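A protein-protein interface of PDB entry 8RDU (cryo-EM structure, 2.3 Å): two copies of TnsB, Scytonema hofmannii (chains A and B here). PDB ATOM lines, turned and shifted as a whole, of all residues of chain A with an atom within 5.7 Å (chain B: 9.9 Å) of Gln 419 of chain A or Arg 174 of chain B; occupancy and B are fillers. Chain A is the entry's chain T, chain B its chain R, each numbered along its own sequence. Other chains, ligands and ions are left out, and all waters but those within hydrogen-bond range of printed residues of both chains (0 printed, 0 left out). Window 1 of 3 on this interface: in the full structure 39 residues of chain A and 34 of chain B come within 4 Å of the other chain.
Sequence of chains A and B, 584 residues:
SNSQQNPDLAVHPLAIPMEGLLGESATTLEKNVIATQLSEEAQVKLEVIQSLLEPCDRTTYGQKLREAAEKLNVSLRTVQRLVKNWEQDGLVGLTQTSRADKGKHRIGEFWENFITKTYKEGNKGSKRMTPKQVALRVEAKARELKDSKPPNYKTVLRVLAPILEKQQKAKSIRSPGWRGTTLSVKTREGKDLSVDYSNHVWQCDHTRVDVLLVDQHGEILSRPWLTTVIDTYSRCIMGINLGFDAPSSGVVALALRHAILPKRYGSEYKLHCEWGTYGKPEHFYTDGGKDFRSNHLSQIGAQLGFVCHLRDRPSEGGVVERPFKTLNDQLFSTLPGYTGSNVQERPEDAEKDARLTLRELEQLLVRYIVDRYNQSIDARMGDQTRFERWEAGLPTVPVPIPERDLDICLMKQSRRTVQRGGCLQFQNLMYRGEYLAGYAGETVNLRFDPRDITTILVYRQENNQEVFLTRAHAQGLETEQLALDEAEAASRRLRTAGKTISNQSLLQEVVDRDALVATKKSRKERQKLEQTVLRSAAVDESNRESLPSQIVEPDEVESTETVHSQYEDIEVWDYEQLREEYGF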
ATOM      1  N   THR A 417     -14.710 -27.808   3.680  1.00  0.00           N
ATOM      2  CA  THR A 417     -14.031 -28.949   3.080  1.00  0.00           C
ATOM      3  C   THR A 417     -12.899 -29.446   3.967  1.00  0.00           C
ATOM      4  O   THR A 417     -12.125 -28.650   4.502  1.00  0.00           O
ATOM      5  CB  THR A 417     -13.464 -28.585   1.720  1.00  0.00           C
ATOM      6  OG1 THR A 417     -12.514 -27.535   1.890  1.00  0.00           O
ATOM      7  CG2 THR A 417     -14.563 -28.095   0.814  1.00  0.00           C
ATOM      8  N   VAL A 418     -12.811 -30.764   4.113  1.00  0.00           N
ATOM      9  CA  VAL A 418     -11.858 -31.396   5.019  1.00  0.00           C
ATOM     10  C   VAL A 418     -10.557 -31.693   4.283  1.00  0.00           C
ATOM     11  O   VAL A 418     -10.544 -32.412   3.279  1.00  0.00           O
ATOM     12  CB  VAL A 418     -12.439 -32.679   5.620  1.00  0.00           C
ATOM     13  CG1 VAL A 418     -11.523 -33.196   6.683  1.00  0.00           C
ATOM     14  CG2 VAL A 418     -13.797 -32.410   6.195  1.00  0.00           C
ATOM     15  N   GLN A 419      -9.462 -31.165   4.807  1.00  0.00           N
ATOM     16  CA  GLN A 419      -8.123 -31.258   4.254  1.00  0.00           C
ATOM     17  C   GLN A 419      -7.399 -32.451   4.873  1.00  0.00           C
ATOM     18  O   GLN A 419      -7.948 -33.155   5.717  1.00  0.00           O
ATOM     19  CB  GLN A 419      -7.389 -29.946   4.483  1.00  0.00           C
ATOM     20  CG  GLN A 419      -8.200 -28.777   3.978  1.00  0.00           C
ATOM     21  CD  GLN A 419      -7.561 -27.457   4.250  1.00  0.00           C
ATOM     22  OE1 GLN A 419      -7.219 -26.719   3.336  1.00  0.00           O
ATOM     23  NE2 GLN A 419      -7.400 -27.137   5.520  1.00  0.00           N
ATOM     24  N   ARG A 420      -6.178 -32.716   4.400  1.00  0.00           N
ATOM     25  CA  ARG A 420      -5.413 -33.858   4.897  1.00  0.00           C
ATOM     26  C   ARG A 420      -5.383 -33.895   6.418  1.00  0.00           C
ATOM     27  O   ARG A 420      -5.231 -32.868   7.080  1.00  0.00           O
ATOM     28  CB  ARG A 420      -3.966 -33.822   4.406  1.00  0.00           C
ATOM     29  CG  ARG A 420      -3.716 -34.342   3.020  1.00  0.00           C
ATOM     30  CD  ARG A 420      -2.248 -34.725   2.850  1.00  0.00           C
ATOM     31  NE  ARG A 420      -1.313 -33.628   3.070  1.00  0.00           N
ATOM     32  CZ  ARG A 420      -0.644 -33.432   4.199  1.00  0.00           C
ATOM     33  NH1 ARG A 420      -0.719 -34.290   5.201  1.00  0.00           N
ATOM     34  NH2 ARG A 420       0.151 -32.372   4.312  1.00  0.00           N
ATOM     35  N   GLY A 421      -5.513 -35.101   6.965  1.00  0.00           N
ATOM     36  CA  GLY A 421      -5.515 -35.291   8.398  1.00  0.00           C
ATOM     37  C   GLY A 421      -6.722 -34.755   9.131  1.00  0.00           C
ATOM     38  O   GLY A 421      -6.686 -34.664  10.359  1.00  0.00           O
ATOM     39  N   GLY A 422      -7.791 -34.403   8.431  1.00  0.00           N
ATOM     40  CA  GLY A 422      -8.974 -33.948   9.125  1.00  0.00           C
ATOM     41  C   GLY A 422      -8.804 -32.521   9.584  1.00  0.00           C
ATOM     42  O   GLY A 422      -8.784 -32.245  10.783  1.00  0.00           O
ATOM     43  N   CYS A 423      -8.641 -31.606   8.642  1.00  0.00           N
ATOM     44  CA  CYS A 423      -8.354 -30.217   8.946  1.00  0.00           C
ATOM     45  C   CYS A 423      -9.386 -29.305   8.291  1.00  0.00           C
ATOM     46  O   CYS A 423      -9.960 -29.641   7.254  1.00  0.00           O
ATOM     47  CB  CYS A 423      -6.943 -29.868   8.475  1.00  0.00           C
ATOM     48  SG  CYS A 423      -6.459 -28.183   8.753  1.00  0.00           S
ATOM     49  N   LEU A 424      -9.653 -28.163   8.923  1.00  0.00           N
ATOM     50  CA  LEU A 424     -10.673 -27.233   8.459  1.00  0.00           C
ATOM     51  C   LEU A 424     -10.175 -25.815   8.665  1.00  0.00           C
ATOM     52  O   LEU A 424      -9.511 -25.524   9.662  1.00  0.00           O
ATOM     53  CB  LEU A 424     -11.990 -27.385   9.214  1.00  0.00           C
ATOM     54  CG  LEU A 424     -12.789 -28.663   9.040  1.00  0.00           C
ATOM     55  CD1 LEU A 424     -13.644 -28.872  10.252  1.00  0.00           C
ATOM     56  CD2 LEU A 424     -13.649 -28.541   7.819  1.00  0.00           C
ATOM     57  N   GLN A 425     -10.539 -24.923   7.753  1.00  0.00           N
ATOM     58  CA  GLN A 425     -10.329 -23.499   7.962  1.00  0.00           C
ATOM     59  C   GLN A 425     -11.609 -22.867   8.486  1.00  0.00           C
ATOM     60  O   GLN A 425     -12.704 -23.216   8.045  1.00  0.00           O
ATOM     61  CB  GLN A 425      -9.895 -22.804   6.675  1.00  0.00           C
ATOM     62  CG  GLN A 425      -9.734 -21.315   6.851  1.00  0.00           C
ATOM     63  CD  GLN A 425      -9.148 -20.652   5.649  1.00  0.00           C
ATOM     64  OE1 GLN A 425      -8.494 -21.293   4.837  1.00  0.00           O
ATOM     65  NE2 GLN A 425      -9.355 -19.355   5.535  1.00  0.00           N
ATOM     66  N   MET A 430      -7.386 -22.125  11.611  1.00  0.00           N
ATOM     67  CA  MET A 430      -7.278 -23.490  11.141  1.00  0.00           C
ATOM     68  C   MET A 430      -7.699 -24.423  12.261  1.00  0.00           C
ATOM     69  O   MET A 430      -7.456 -24.137  13.434  1.00  0.00           O
ATOM     70  CB  MET A 430      -5.854 -23.777  10.690  1.00  0.00           C
ATOM     71  CG  MET A 430      -5.677 -25.061   9.926  1.00  0.00           C
ATOM     72  SD  MET A 430      -6.305 -24.922   8.243  1.00  0.00           S
ATOM     73  CE  MET A 430      -5.188 -23.715   7.561  1.00  0.00           C
ATOM     74  N   LEU A 436     -11.877 -36.766  12.228  1.00  0.00           N
ATOM     75  CA  LEU A 436     -12.200 -36.095  10.980  1.00  0.00           C
ATOM     76  C   LEU A 436     -11.261 -36.488   9.844  1.00  0.00           C
ATOM     77  O   LEU A 436     -11.615 -36.323   8.673  1.00  0.00           O
ATOM     78  CB  LEU A 436     -12.144 -34.589  11.219  1.00  0.00           C
ATOM     79  CG  LEU A 436     -12.549 -33.666  10.083  1.00  0.00           C
ATOM     80  CD1 LEU A 436     -13.986 -33.941   9.710  1.00  0.00           C
ATOM     81  CD2 LEU A 436     -12.360 -32.224  10.474  1.00  0.00           C
ATOM     82  N   ALA A 437     -10.078 -37.017  10.161  1.00  0.00           N
ATOM     83  CA  ALA A 437      -9.162 -37.489   9.130  1.00  0.00           C
ATOM     84  C   ALA A 437      -9.742 -38.604   8.270  1.00  0.00           C
ATOM     85  O   ALA A 437      -9.271 -38.805   7.147  1.00  0.00           O
ATOM     86  CB  ALA A 437      -7.859 -37.963   9.772  1.00  0.00           C
ATOM     87  N   ALA A 440     -11.238 -36.635   5.123  1.00  0.00           N
ATOM     88  CA  ALA A 440     -10.492 -35.706   4.289  1.00  0.00           C
ATOM     89  C   ALA A 440     -10.964 -35.797   2.845  1.00  0.00           C
ATOM     90  O   ALA A 440     -11.294 -36.876   2.348  1.00  0.00           O
ATOM     91  CB  ALA A 440      -8.997 -35.998   4.375  1.00  0.00           C
ATOM     92  N   GLY A 441     -10.999 -34.644   2.174  1.00  0.00           N
ATOM     93  CA  GLY A 441     -11.590 -34.507   0.857  1.00  0.00           C
ATOM     94  C   GLY A 441     -13.101 -34.439   0.815  1.00  0.00           C
ATOM     95  O   GLY A 441     -13.657 -34.037  -0.212  1.00  0.00           O
ATOM     96  N   LYS B 169     -11.944 -39.297  -5.781  1.00  0.00           N
ATOM     97  CA  LYS B 169     -11.732 -38.364  -4.674  1.00  0.00           C
ATOM     98  C   LYS B 169     -10.257 -38.219  -4.306  1.00  0.00           C
ATOM     99  O   LYS B 169      -9.811 -37.136  -3.910  1.00  0.00           O
ATOM    100  CB  LYS B 169     -12.535 -38.812  -3.456  1.00  0.00           C
ATOM    101  CG  LYS B 169     -12.600 -37.760  -2.370  1.00  0.00           C
ATOM    102  CD  LYS B 169     -13.217 -38.303  -1.099  1.00  0.00           C
ATOM    103  CE  LYS B 169     -12.341 -39.377  -0.484  1.00  0.00           C
ATOM    104  NZ  LYS B 169     -12.676 -39.619   0.940  1.00  0.00           N
ATOM    105  N   ALA B 170      -9.490 -39.304  -4.420  1.00  0.00           N
ATOM    106  CA  ALA B 170      -8.064 -39.283  -4.105  1.00  0.00           C
ATOM    107  C   ALA B 170      -7.288 -38.199  -4.848  1.00  0.00           C
ATOM    108  O   ALA B 170      -6.245 -37.749  -4.366  1.00  0.00           O
ATOM    109  CB  ALA B 170      -7.453 -40.652  -4.403  1.00  0.00           C
ATOM    110  N   LYS B 171      -7.777 -37.755  -6.006  1.00  0.00           N
ATOM    111  CA  LYS B 171      -7.094 -36.689  -6.737  1.00  0.00           C
ATOM    112  C   LYS B 171      -7.232 -35.315  -6.092  1.00  0.00           C
ATOM    113  O   LYS B 171      -6.423 -34.430  -6.385  1.00  0.00           O
ATOM    114  CB  LYS B 171      -7.610 -36.613  -8.176  1.00  0.00           C
ATOM    115  CG  LYS B 171      -7.128 -37.720  -9.107  1.00  0.00           C
ATOM    116  CD  LYS B 171      -8.051 -38.925  -9.087  1.00  0.00           C
ATOM    117  CE  LYS B 171      -7.549 -40.029 -10.005  1.00  0.00           C
ATOM    118  NZ  LYS B 171      -8.497 -41.177 -10.064  1.00  0.00           N
ATOM    119  N   SER B 172      -8.229 -35.105  -5.236  1.00  0.00           N
ATOM    120  CA  SER B 172      -8.622 -33.765  -4.815  1.00  0.00           C
ATOM    121  C   SER B 172      -8.143 -33.381  -3.417  1.00  0.00           C
ATOM    122  O   SER B 172      -8.115 -32.189  -3.101  1.00  0.00           O
ATOM    123  CB  SER B 172     -10.144 -33.622  -4.874  1.00  0.00           C
ATOM    124  OG  SER B 172     -10.520 -32.256  -4.853  1.00  0.00           O
ATOM    125  N   ILE B 173      -7.763 -34.357  -2.591  1.00  0.00           N
ATOM    126  CA  ILE B 173      -7.497 -34.143  -1.170  1.00  0.00           C
ATOM    127  C   ILE B 173      -6.432 -33.077  -0.953  1.00  0.00           C
ATOM    128  O   ILE B 173      -5.273 -33.241  -1.348  1.00  0.00           O
ATOM    129  CB  ILE B 173      -7.084 -35.463  -0.519  1.00  0.00           C
ATOM    130  CG1 ILE B 173      -8.212 -36.486  -0.643  1.00  0.00           C
ATOM    131  CG2 ILE B 173      -6.733 -35.250   0.926  1.00  0.00           C
ATOM    132  CD1 ILE B 173      -7.785 -37.904  -0.341  1.00  0.00           C
ATOM    133  N   ARG B 174      -6.828 -31.976  -0.316  1.00  0.00           N
ATOM    134  CA  ARG B 174      -5.995 -30.796  -0.125  1.00  0.00           C
ATOM    135  C   ARG B 174      -5.058 -30.963   1.069  1.00  0.00           C
ATOM    136  O   ARG B 174      -5.354 -31.683   2.022  1.00  0.00           O
ATOM    137  CB  ARG B 174      -6.873 -29.563   0.072  1.00  0.00           C
ATOM    138  CG  ARG B 174      -6.137 -28.248   0.100  1.00  0.00           C
ATOM    139  CD  ARG B 174      -7.110 -27.108   0.084  1.00  0.00           C
ATOM    140  NE  ARG B 174      -6.490 -25.833  -0.242  1.00  0.00           N
ATOM    141  CZ  ARG B 174      -5.992 -25.005   0.663  1.00  0.00           C
ATOM    142  NH1 ARG B 174      -5.980 -25.315   1.944  1.00  0.00           N
ATOM    143  NH2 ARG B 174      -5.492 -23.837   0.274  1.00  0.00           N
ATOM    144  N   SER B 175      -3.896 -30.289   0.998  1.00  0.00           N
ATOM    145  CA  SER B 175      -2.906 -30.207   2.072  1.00  0.00           C
ATOM    146  C   SER B 175      -3.035 -28.904   2.848  1.00  0.00           C
ATOM    147  O   SER B 175      -3.052 -27.829   2.236  1.00  0.00           O
ATOM    148  CB  SER B 175      -1.500 -30.320   1.498  1.00  0.00           C
ATOM    149  OG  SER B 175      -1.199 -31.659   1.152  1.00  0.00           O
ATOM    150  N   PRO B 176      -3.121 -28.964   4.179  1.00  0.00           N
ATOM    151  CA  PRO B 176      -3.313 -27.737   4.973  1.00  0.00           C
ATOM    152  C   PRO B 176      -2.241 -26.680   4.780  1.00  0.00           C
ATOM    153  O   PRO B 176      -2.559 -25.487   4.743  1.00  0.00           O
ATOM    154  CB  PRO B 176      -3.306 -28.262   6.410  1.00  0.00           C
ATOM    155  CG  PRO B 176      -3.755 -29.660   6.294  1.00  0.00           C
ATOM    156  CD  PRO B 176      -3.231 -30.175   4.999  1.00  0.00           C
ATOM    157  N   GLY B 177      -0.983 -27.084   4.659  1.00  0.00           N
ATOM    158  CA  GLY B 177       0.143 -26.173   4.627  1.00  0.00           C
ATOM    159  C   GLY B 177       0.585 -25.678   5.995  1.00  0.00           C
ATOM    160  O   GLY B 177      -0.110 -25.799   6.996  1.00  0.00           O
ATOM    161  N   TRP B 178       1.793 -25.123   6.021  1.00  0.00           N
ATOM    162  CA  TRP B 178       2.309 -24.442   7.199  1.00  0.00           C
ATOM    163  C   TRP B 178       1.607 -23.118   7.426  1.00  0.00           C
ATOM    164  O   TRP B 178       1.096 -22.488   6.501  1.00  0.00           O
ATOM    165  CB  TRP B 178       3.826 -24.237   7.097  1.00  0.00           C
ATOM    166  CG  TRP B 178       4.589 -25.448   7.511  1.00  0.00           C
ATOM    167  CD1 TRP B 178       4.871 -26.537   6.751  1.00  0.00           C
ATOM    168  CD2 TRP B 178       5.152 -25.700   8.797  1.00  0.00           C
ATOM    169  NE1 TRP B 178       5.572 -27.458   7.482  1.00  0.00           N
ATOM    170  CE2 TRP B 178       5.758 -26.965   8.746  1.00  0.00           C
ATOM    171  CE3 TRP B 178       5.202 -24.980   9.989  1.00  0.00           C
ATOM    172  CZ2 TRP B 178       6.408 -27.523   9.839  1.00  0.00           C
ATOM    173  CZ3 TRP B 178       5.847 -25.532  11.068  1.00  0.00           C
ATOM    174  CH2 TRP B 178       6.439 -26.791  10.989  1.00  0.00           C
ATOM    175  N   ARG B 179       1.578 -22.709   8.687  1.00  0.00           N
ATOM    176  CA  ARG B 179       0.836 -21.547   9.133  1.00  0.00           C
ATOM    177  C   ARG B 179       1.760 -20.665   9.960  1.00  0.00           C
ATOM    178  O   ARG B 179       2.703 -21.151  10.586  1.00  0.00           O
ATOM    179  CB  ARG B 179      -0.366 -21.979   9.971  1.00  0.00           C
ATOM    180  CG  ARG B 179      -1.461 -22.735   9.221  1.00  0.00           C
ATOM    181  CD  ARG B 179      -2.233 -21.856   8.278  1.00  0.00           C
ATOM    182  NE  ARG B 179      -2.827 -20.737   8.996  1.00  0.00           N
ATOM    183  CZ  ARG B 179      -3.903 -20.072   8.600  1.00  0.00           C
ATOM    184  NH1 ARG B 179      -4.535 -20.383   7.482  1.00  0.00           N
ATOM    185  NH2 ARG B 179      -4.351 -19.065   9.343  1.00  0.00           N
ATOM    186  N   ARG B 322       6.680 -23.480  -6.042  1.00  0.00           N
ATOM    187  CA  ARG B 322       5.541 -22.605  -6.274  1.00  0.00           C
ATOM    188  C   ARG B 322       5.839 -21.313  -7.027  1.00  0.00           C
ATOM    189  O   ARG B 322       5.066 -20.954  -7.918  1.00  0.00           O
ATOM    190  CB  ARG B 322       4.841 -22.281  -4.955  1.00  0.00           C
ATOM    191  CG  ARG B 322       3.641 -21.386  -5.160  1.00  0.00           C
ATOM    192  CD  ARG B 322       2.683 -21.944  -6.190  1.00  0.00           C
ATOM    193  NE  ARG B 322       1.823 -20.876  -6.679  1.00  0.00           N
ATOM    194  CZ  ARG B 322       0.506 -20.874  -6.602  1.00  0.00           C
ATOM    195  NH1 ARG B 322      -0.143 -21.829  -5.975  1.00  0.00           N
ATOM    196  NH2 ARG B 322      -0.171 -19.856  -7.119  1.00  0.00           N
ATOM    197  N   ALA B 379       2.441 -14.815   1.840  1.00  0.00           N
ATOM    198  CA  ALA B 379       1.111 -15.387   1.976  1.00  0.00           C
ATOM    199  C   ALA B 379       0.844 -16.058   3.320  1.00  0.00           C
ATOM    200  O   ALA B 379      -0.307 -16.415   3.582  1.00  0.00           O
ATOM    201  CB  ALA B 379       0.873 -16.400   0.867  1.00  0.00           C
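NZ of Lys 169 of chain B is in hydrogen-bond range of O of Ala 440 of chain A, at 3.4 Å. The backbone NH (N) of Arg 420 of chain A sits at hydrogen-bond distance from the backbone carbonyl oxygen (O) of Arg 174 of chain B (2.7 Å). The side-chain hydroxyl (OG) of Ser 175 of chain B sits at hydrogen-bond distance from the guanidinium group (NE) of Arg 420 of chain A (2.8 Å). OE1 of Gln 419 of chain A lies close to NH1 of Arg 174 of chain B, at 2.3 Å.
No position is printed for both chains. Of the 8 pairs that touch across the chains among the printed residues, none has its exchanged pair printed and touching as well.
Among the printed residues, merely in contact across the chains: Met 430 of chain A with Arg 179 of chain B (3.4 Å), Arg 420 of chain A with Pro 176 of chain B (3.6 Å), Arg 420 of chain A with Ile 173 of chain B (3.8 Å) and Cys 423 of chain A with Pro 176 of chain B (3.9 Å).
Thr 417 of chain A touches none of the printed residues of chain B. Val 418 of chain A touches none of the printed residues of chain B. No residue of chain B comes within 4 Å of Gly 421 of chain A. No residue of chain B comes within 4 Å of Gly 422 of chain A. Of the printed residues of chain B, Cys 423 of chain A touches Pro 176. Ala 170 of chain B touches none of the printed residues of chain A. Arg 174 of chain B touches two residues of chain A. Printed residues of chain A within 4 Å of Pro 176 of chain B: Arg 420 and Cys 423. Of the printed residues of chain A, Arg 179 of chain B touches Met 430. The nearest residue of chain B that does not touch Gln 419 of chain A is Pro 176 of chain B (4.1 Å). The nearest residue of chain A that does not touch Arg 174 of chain B is Val 418 of chain A (5.2 Å).
Printed residues of chain A that touch a printed residue of chain B: Gln 419, Arg 420, Cys 423, Met 430 and Ala 440. Along chain A the printed residues that touch a printed residue of chain B span positions 419 to 440. Among the printed residues, no Asp or Glu carboxylate lies within 4 Å of a Lys or Arg side-chain nitrogen of the other chain.
The side-chain amide nitrogen of Gln 419 of chain A lies within hydrogen-bond range of the side-chain sulfur of Cys 423 of chain A, at 3.5 Å. NE2 of Gln 419 of chain A sits at hydrogen-bond distance from SD of Met 430 of chain A (3.7 Å). The side-chain sulfur of Met 430 of chain A lies within hydrogen-bond range of the side-chain sulfur of Cys 423 of chain A, at 3.3 Å.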
